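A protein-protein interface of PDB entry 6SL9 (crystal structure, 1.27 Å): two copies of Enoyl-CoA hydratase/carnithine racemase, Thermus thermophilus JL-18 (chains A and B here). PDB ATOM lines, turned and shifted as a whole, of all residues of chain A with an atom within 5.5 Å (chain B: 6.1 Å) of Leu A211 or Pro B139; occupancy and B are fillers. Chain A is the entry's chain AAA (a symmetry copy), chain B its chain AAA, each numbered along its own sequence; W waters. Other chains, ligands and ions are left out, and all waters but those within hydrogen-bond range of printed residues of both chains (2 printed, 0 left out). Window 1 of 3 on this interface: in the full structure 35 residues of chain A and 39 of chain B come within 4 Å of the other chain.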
ATOM      1  N   LEU A 207      30.281  27.279  11.496  1.00  0.00           N
ATOM      2  CA  LEU A 207      29.606  25.965  11.464  1.00  0.00           C
ATOM      3  C   LEU A 207      30.195  25.092  10.356  1.00  0.00           C
ATOM      4  O   LEU A 207      30.330  23.880  10.530  1.00  0.00           O
ATOM      5  CB  LEU A 207      28.093  26.151  11.367  1.00  0.00           C
ATOM      6  CG  LEU A 207      27.459  26.872  12.553  1.00  0.00           C
ATOM      7  CD1 LEU A 207      26.026  27.176  12.280  1.00  0.00           C
ATOM      8  CD2 LEU A 207      27.550  26.089  13.815  1.00  0.00           C
ATOM      9  N   THR A 208      30.581  25.697   9.240  1.00  0.00           N
ATOM     10  CA  THR A 208      31.265  24.961   8.158  1.00  0.00           C
ATOM     11  C   THR A 208      32.585  24.401   8.666  1.00  0.00           C
ATOM     12  O   THR A 208      32.920  23.240   8.364  1.00  0.00           O
ATOM     13  CB  THR A 208      31.431  25.846   6.921  1.00  0.00           C
ATOM     14  OG1 THR A 208      30.140  26.230   6.454  1.00  0.00           O
ATOM     15  CG2 THR A 208      32.148  25.143   5.810  1.00  0.00           C
ATOM     16  N   LYS A 209      33.308  25.175   9.424  1.00  0.00           N
ATOM     17  CA  LYS A 209      34.608  24.718   9.982  1.00  0.00           C
ATOM     18  C   LYS A 209      34.400  23.496  10.861  1.00  0.00           C
ATOM     19  O   LYS A 209      35.224  22.571  10.823  1.00  0.00           O
ATOM     20  CB  LYS A 209      35.256  25.852  10.770  1.00  0.00           C
ATOM     21  CG  LYS A 209      35.828  26.914   9.867  1.00  0.00           C
ATOM     22  CD  LYS A 209      36.293  28.107  10.659  1.00  0.00           C
ATOM     23  CE  LYS A 209      37.362  27.768  11.689  1.00  0.00           C
ATOM     24  NZ  LYS A 209      38.187  28.983  12.009  1.00  0.00           N
ATOM     25  N   LYS A 210      33.317  23.452  11.615  1.00  0.00           N
ATOM     26  CA  LYS A 210      33.010  22.310  12.488  1.00  0.00           C
ATOM     27  C   LYS A 210      32.763  21.070  11.652  1.00  0.00           C
ATOM     28  O   LYS A 210      33.255  19.988  11.992  1.00  0.00           O
ATOM     29  CB  LYS A 210      31.791  22.644  13.347  1.00  0.00           C
ATOM     30  CG  LYS A 210      31.983  23.729  14.386  1.00  0.00           C
ATOM     31  CD  LYS A 210      30.818  23.945  15.403  1.00  0.00           C
ATOM     32  CE  LYS A 210      30.956  25.335  16.028  1.00  0.00           C
ATOM     33  NZ  LYS A 210      32.251  25.512  16.777  1.00  0.00           N
ATOM     34  N   LEU A 211      31.981  21.199  10.580  1.00  0.00           N
ATOM     35  CA  LEU A 211      31.730  20.053   9.692  1.00  0.00           C
ATOM     36  C   LEU A 211      33.019  19.527   9.092  1.00  0.00           C
ATOM     37  O   LEU A 211      33.219  18.315   9.034  1.00  0.00           O
ATOM     38  CB  LEU A 211      30.775  20.462   8.597  1.00  0.00           C
ATOM     39  CG  LEU A 211      29.345  20.683   9.037  1.00  0.00           C
ATOM     40  CD1 LEU A 211      28.572  21.373   7.912  1.00  0.00           C
ATOM     41  CD2 LEU A 211      28.641  19.375   9.385  1.00  0.00           C
ATOM     42  N   LEU A 212      33.878  20.429   8.659  1.00  0.00           N
ATOM     43  CA  LEU A 212      35.156  20.006   8.068  1.00  0.00           C
ATOM     44  C   LEU A 212      36.025  19.324   9.092  1.00  0.00           C
ATOM     45  O   LEU A 212      36.660  18.312   8.748  1.00  0.00           O
ATOM     46  CB  LEU A 212      35.873  21.200   7.465  1.00  0.00           C
ATOM     47  CG  LEU A 212      35.233  21.775   6.188  1.00  0.00           C
ATOM     48  CD1 LEU A 212      35.983  23.017   5.774  1.00  0.00           C
ATOM     49  CD2 LEU A 212      35.205  20.717   5.085  1.00  0.00           C
ATOM     50  N   LEU A 213      36.073  19.798  10.309  1.00  0.00           N
ATOM     51  CA  LEU A 213      36.986  19.225  11.325  1.00  0.00           C
ATOM     52  C   LEU A 213      36.586  17.762  11.611  1.00  0.00           C
ATOM     53  O   LEU A 213      37.431  16.956  11.941  1.00  0.00           O
ATOM     54  CB  LEU A 213      36.984  20.060  12.600  1.00  0.00           C
ATOM     55  CG  LEU A 213      38.126  19.802  13.551  1.00  0.00           C
ATOM     56  CD1 LEU A 213      39.426  20.290  12.978  1.00  0.00           C
ATOM     57  CD2 LEU A 213      37.883  20.430  14.890  1.00  0.00           C
ATOM     58  N   GLU A 214      35.295  17.458  11.521  1.00  0.00           N
ATOM     59  CA  GLU A 214      34.779  16.103  11.882  1.00  0.00           C
ATOM     60  C   GLU A 214      34.705  15.170  10.673  1.00  0.00           C
ATOM     61  O   GLU A 214      34.444  13.983  10.918  1.00  0.00           O
ATOM     62  CB  GLU A 214      33.381  16.199  12.476  1.00  0.00           C
ATOM     63  CG  GLU A 214      33.350  17.080  13.701  1.00  0.00           C
ATOM     64  CD  GLU A 214      32.393  16.642  14.770  1.00  0.00           C
ATOM     65  OE1 GLU A 214      31.658  17.538  15.266  1.00  0.00           O
ATOM     66  OE2 GLU A 214      32.527  15.447  15.199  1.00  0.00           O
ATOM     67  N   THR A 215      34.751  15.655   9.430  1.00  0.00           N
ATOM     68  CA  THR A 215      34.227  14.911   8.221  1.00  0.00           C
ATOM     69  C   THR A 215      34.842  13.505   8.147  1.00  0.00           C
ATOM     70  O   THR A 215      34.154  12.495   7.772  1.00  0.00           O
ATOM     71  CB  THR A 215      34.461  15.711   6.928  1.00  0.00           C
ATOM     72  OG1 THR A 215      33.805  14.902   5.886  1.00  0.00           O
ATOM     73  CG2 THR A 215      35.948  15.953   6.688  1.00  0.00           C
ATOM     74  N   ALA A 223      27.349  12.104   9.467  1.00  0.00           N
ATOM     75  CA  ALA A 223      27.629  13.383   8.806  1.00  0.00           C
ATOM     76  C   ALA A 223      26.317  14.029   8.374  1.00  0.00           C
ATOM     77  O   ALA A 223      26.139  15.249   8.534  1.00  0.00           O
ATOM     78  CB  ALA A 223      28.528  13.186   7.628  1.00  0.00           C
ATOM     79  N   LEU A 226      24.643  15.536  11.393  1.00  0.00           N
ATOM     80  CA  LEU A 226      25.349  16.748  11.873  1.00  0.00           C
ATOM     81  C   LEU A 226      25.063  17.909  10.921  1.00  0.00           C
ATOM     82  O   LEU A 226      24.830  19.034  11.390  1.00  0.00           O
ATOM     83  CB  LEU A 226      26.852  16.504  12.000  1.00  0.00           C
ATOM     84  CG  LEU A 226      27.667  17.665  12.571  1.00  0.00           C
ATOM     85  CD1 LEU A 226      27.182  18.019  13.956  1.00  0.00           C
ATOM     86  CD2 LEU A 226      29.135  17.308  12.565  1.00  0.00           C
ATOM     87  N   GLU A 227      25.061  17.632   9.611  1.00  0.00           N
ATOM     88  CA  GLU A 227      24.632  18.654   8.643  1.00  0.00           C
ATOM     89  C   GLU A 227      23.235  19.175   8.983  1.00  0.00           C
ATOM     90  O   GLU A 227      22.976  20.386   8.952  1.00  0.00           O
ATOM     91  CB  GLU A 227      24.683  18.108   7.228  1.00  0.00           C
ATOM     92  CG  GLU A 227      26.054  17.938   6.616  1.00  0.00           C
ATOM     93  CD  GLU A 227      26.098  17.305   5.229  1.00  0.00           C
ATOM     94  OE1 GLU A 227      27.190  17.235   4.593  1.00  0.00           O
ATOM     95  OE2 GLU A 227      25.007  16.846   4.792  1.00  0.00           O
ATOM     96  N   LEU A 230      23.443  21.440  12.190  1.00  0.00           N
ATOM     97  CA  LEU A 230      24.118  22.734  12.010  1.00  0.00           C
ATOM     98  C   LEU A 230      23.379  23.585  10.992  1.00  0.00           C
ATOM     99  O   LEU A 230      23.360  24.793  11.145  1.00  0.00           O
ATOM    100  CB  LEU A 230      25.584  22.480  11.675  1.00  0.00           C
ATOM    101  CG  LEU A 230      26.405  21.712  12.742  1.00  0.00           C
ATOM    102  CD1 LEU A 230      27.876  21.658  12.383  1.00  0.00           C
ATOM    103  CD2 LEU A 230      26.239  22.288  14.147  1.00  0.00           C
ATOM    104  N   GLN A 231      22.830  22.973   9.943  1.00  0.00           N
ATOM    105  CA  GLN A 231      22.008  23.772   9.026  1.00  0.00           C
ATOM    106  C   GLN A 231      20.783  24.317   9.753  1.00  0.00           C
ATOM    107  O   GLN A 231      20.348  25.447   9.435  1.00  0.00           O
ATOM    108  CB  GLN A 231      21.571  22.965   7.821  1.00  0.00           C
ATOM    109  CG  GLN A 231      21.024  23.783   6.658  1.00  0.00           C
ATOM    110  CD  GLN A 231      22.159  24.508   5.956  1.00  0.00           C
ATOM    111  OE1 GLN A 231      22.819  25.412   6.525  1.00  0.00           O
ATOM    112  NE2 GLN A 231      22.459  24.017   4.763  1.00  0.00           N
ATOM    113  N   SER B 112      25.972  18.900  -4.515  1.00  0.00           N
ATOM    114  CA  SER B 112      25.951  17.701  -3.659  1.00  0.00           C
ATOM    115  C   SER B 112      25.492  16.479  -4.436  1.00  0.00           C
ATOM    116  O   SER B 112      26.176  15.432  -4.421  1.00  0.00           O
ATOM    117  CB  SER B 112      25.071  17.907  -2.423  1.00  0.00           C
ATOM    118  OG  SER B 112      25.377  19.118  -1.719  1.00  0.00           O
ATOM    119  N   PHE B 132      26.184  27.493  -0.817  1.00  0.00           N
ATOM    120  CA  PHE B 132      25.496  27.593   0.490  1.00  0.00           C
ATOM    121  C   PHE B 132      25.947  28.845   1.247  1.00  0.00           C
ATOM    122  O   PHE B 132      25.081  29.547   1.844  1.00  0.00           O
ATOM    123  CB  PHE B 132      25.787  26.355   1.351  1.00  0.00           C
ATOM    124  CG  PHE B 132      25.119  25.111   0.818  1.00  0.00           C
ATOM    125  CD1 PHE B 132      23.813  24.856   1.125  1.00  0.00           C
ATOM    126  CD2 PHE B 132      25.834  24.153   0.100  1.00  0.00           C
ATOM    127  CE1 PHE B 132      23.201  23.708   0.709  1.00  0.00           C
ATOM    128  CE2 PHE B 132      25.214  22.974  -0.307  1.00  0.00           C
ATOM    129  CZ  PHE B 132      23.910  22.783  -0.002  1.00  0.00           C
ATOM    130  N   LEU B 137      24.449  29.732   4.740  1.00  0.00           N
ATOM    131  CA  LEU B 137      24.214  28.334   5.141  1.00  0.00           C
ATOM    132  C   LEU B 137      25.504  27.535   5.077  1.00  0.00           C
ATOM    133  O   LEU B 137      26.505  27.987   4.543  1.00  0.00           O
ATOM    134  CB  LEU B 137      23.133  27.752   4.233  1.00  0.00           C
ATOM    135  CG  LEU B 137      21.711  28.305   4.384  1.00  0.00           C
ATOM    136  CD1 LEU B 137      20.745  27.480   3.536  1.00  0.00           C
ATOM    137  CD2 LEU B 137      21.219  28.306   5.840  1.00  0.00           C
ATOM    138  N   VAL B 138      25.421  26.345   5.633  1.00  0.00           N
ATOM    139  CA  VAL B 138      26.532  25.365   5.597  1.00  0.00           C
ATOM    140  C   VAL B 138      26.304  24.353   4.490  1.00  0.00           C
ATOM    141  O   VAL B 138      25.171  24.204   3.999  1.00  0.00           O
ATOM    142  CB  VAL B 138      26.649  24.649   6.956  1.00  0.00           C
ATOM    143  CG1 VAL B 138      26.789  25.612   8.107  1.00  0.00           C
ATOM    144  CG2 VAL B 138      25.518  23.644   7.197  1.00  0.00           C
ATOM    145  N   PRO B 139      27.318  23.586   4.082  1.00  0.00           N
ATOM    146  CA  PRO B 139      27.096  22.519   3.120  1.00  0.00           C
ATOM    147  C   PRO B 139      26.149  21.472   3.697  1.00  0.00           C
ATOM    148  O   PRO B 139      26.301  21.059   4.827  1.00  0.00           O
ATOM    149  CB  PRO B 139      28.484  21.973   2.912  1.00  0.00           C
ATOM    150  CG  PRO B 139      29.306  22.382   4.060  1.00  0.00           C
ATOM    151  CD  PRO B 139      28.739  23.721   4.427  1.00  0.00           C
ATOM    152  N   ASP B 140      25.210  21.005   2.867  1.00  0.00           N
ATOM    153  CA  ASP B 140      24.318  19.910   3.270  1.00  0.00           C
ATOM    154  C   ASP B 140      24.227  18.879   2.160  1.00  0.00           C
ATOM    155  O   ASP B 140      24.930  18.950   1.143  1.00  0.00           O
ATOM    156  CB  ASP B 140      22.989  20.454   3.825  1.00  0.00           C
ATOM    157  CG  ASP B 140      22.002  21.040   2.830  1.00  0.00           C
ATOM    158  OD1 ASP B 140      22.009  20.626   1.639  1.00  0.00           O
ATOM    159  OD2 ASP B 140      21.220  21.923   3.269  1.00  0.00           O
ATOM    160  N   SER B 141      23.309  17.939   2.351  1.00  0.00           N
ATOM    161  CA  SER B 141      23.056  16.863   1.393  1.00  0.00           C
ATOM    162  C   SER B 141      24.331  16.059   1.129  1.00  0.00           C
ATOM    163  O   SER B 141      24.511  15.485   0.007  1.00  0.00           O
ATOM    164  CB  SER B 141      22.426  17.418   0.119  1.00  0.00           C
ATOM    165  OG  SER B 141      21.333  18.249   0.408  1.00  0.00           O
ATOM    166  N   GLY B 142      25.176  15.922   2.135  1.00  0.00           N
ATOM    167  CA  GLY B 142      26.395  15.154   2.060  1.00  0.00           C
ATOM    168  C   GLY B 142      27.593  15.903   1.490  1.00  0.00           C
ATOM    169  O   GLY B 142      28.660  15.272   1.404  1.00  0.00           O
ATOM    170  N   LEU B 143      27.441  17.188   1.160  1.00  0.00           N
ATOM    171  CA  LEU B 143      28.590  17.879   0.533  1.00  0.00           C
ATOM    172  C   LEU B 143      29.728  17.977   1.559  1.00  0.00           C
ATOM    173  O   LEU B 143      30.915  17.967   1.132  1.00  0.00           O
ATOM    174  CB  LEU B 143      28.164  19.251   0.051  1.00  0.00           C
ATOM    175  CG  LEU B 143      29.245  20.027  -0.735  1.00  0.00           C
ATOM    176  CD1 LEU B 143      29.667  19.252  -1.960  1.00  0.00           C
ATOM    177  CD2 LEU B 143      28.687  21.386  -1.097  1.00  0.00           C
ATOM    178  N   SER B 144      29.446  18.115   2.869  1.00  0.00           N
ATOM    179  CA  SER B 144      30.555  18.236   3.832  1.00  0.00           C
ATOM    180  C   SER B 144      31.332  16.907   3.959  1.00  0.00           C
ATOM    181  O   SER B 144      32.477  16.950   4.394  1.00  0.00           O
ATOM    182  CB  SER B 144      30.090  18.710   5.178  1.00  0.00           C
ATOM    183  OG  SER B 144      29.425  17.712   5.923  1.00  0.00           O
ATOM    184  N   LEU B 160      34.347  25.902  -0.155  1.00  0.00           N
ATOM    185  CA  LEU B 160      33.190  26.112   0.711  1.00  0.00           C
ATOM    186  C   LEU B 160      33.136  27.523   1.283  1.00  0.00           C
ATOM    187  O   LEU B 160      32.029  28.127   1.342  1.00  0.00           O
ATOM    188  CB  LEU B 160      33.200  25.065   1.838  1.00  0.00           C
ATOM    189  CG  LEU B 160      32.889  23.659   1.387  1.00  0.00           C
ATOM    190  CD1 LEU B 160      33.268  22.698   2.487  1.00  0.00           C
ATOM    191  CD2 LEU B 160      31.417  23.493   1.015  1.00  0.00           C
HETATM  192  O   HOH W   1      29.147  27.177   3.863  1.00  0.00           O
HETATM  193  O   HOH W   2      22.207  17.089   4.853  1.00  0.00           O
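O of Ser B144 sits at hydrogen-bond distance from OG1 of Thr A215.
The backbone NH (N) of Ser B141 is in hydrogen-bond range of the side-chain carboxylate (OE2) of Glu A227 (3.2 Å).
The side-chain carboxylate (OD2) of Asp B140 sits at hydrogen-bond distance from the side-chain amide nitrogen (NE2) of Gln A231, at 2.9 Å.
The backbone carbonyl oxygen of Val B138 sits at hydrogen-bond distance from the side-chain amide nitrogen of Gln A231, 2.8 Å away.
N of Leu B143 lies within hydrogen-bond range of OE1 of Glu A227.
The side-chain carboxylate (OE2) of Glu A227 lies within hydrogen-bond range of the backbone NH (N) of Gly B142 (2.8 Å).
OE1 of Glu A227 sits at hydrogen-bond distance from OG of Ser B144 (2.6 Å).
The backbone carbonyl oxygen of Phe B132 sits at hydrogen-bond distance from the backbone NH of Leu B137 (3.0 Å).
OG of Ser B112 sits at hydrogen-bond distance from O of Asp B140, 2.9 Å away.
OD1 of Asp B140 is in hydrogen-bond range of OG of Ser B141, at 2.8 Å.
Among the printed residues, pairs that only touch across the chains: Gln A231 with Leu B137 (3.3 Å), Glu A227 with Asp B140 (3.4 Å), Thr A208 with Pro B139 (3.5 Å), Leu A207 with Val B138 (3.6 Å), Glu A227 with Pro B139 (3.6 Å), Thr A208 with Val B138 (3.8 Å), Leu A212 with Leu B160 (3.8 Å), Leu A211 with Pro B139 (3.8 Å), Leu A211 with Val B138 (3.9 Å), Leu A211 with Ser B144 (3.9 Å) and Gln A231 with Phe B132 (3.97 Å).
Lys A210 touches none of the printed residues of chain B.
Leu A211 touches just these residues of chain B: Val B138, Pro B139 and Ser B144.
Leu A213 touches none of the printed residues of chain B.
Pro B139 touches just these residues of chain A: Thr A208, Leu A211 and Glu A227.
Printed residues of chain A within 4 Å of Leu B143: Glu A227.
Of the printed residues of chain A, Leu B160 touches Leu A212 (3.8 Å).
Printed residues of chain A that touch a printed residue of chain B: Leu A207, Thr A208, Leu A211, Leu A212, Thr A215, Glu A227 and Gln A231.
Hydrophobic or aromatic side chains of chain A that line the printed part of chain B: Leu A207, Leu A211 and Leu A212.
Among the printed residues, 18 pairs touch across the chains.
Among the printed residues, no Asp or Glu carboxylate lies within 4 Å of a Lys or Arg side-chain nitrogen of the other chain.
No position is printed for both chains.
Water W2 lies within hydrogen-bond range of the side-chain carboxylate of Glu A227 and the backbone NH of Ser B141.
Water W1 bridges the backbone carbonyl oxygen of Leu B137 and the side-chain hydroxyl of Thr A208.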
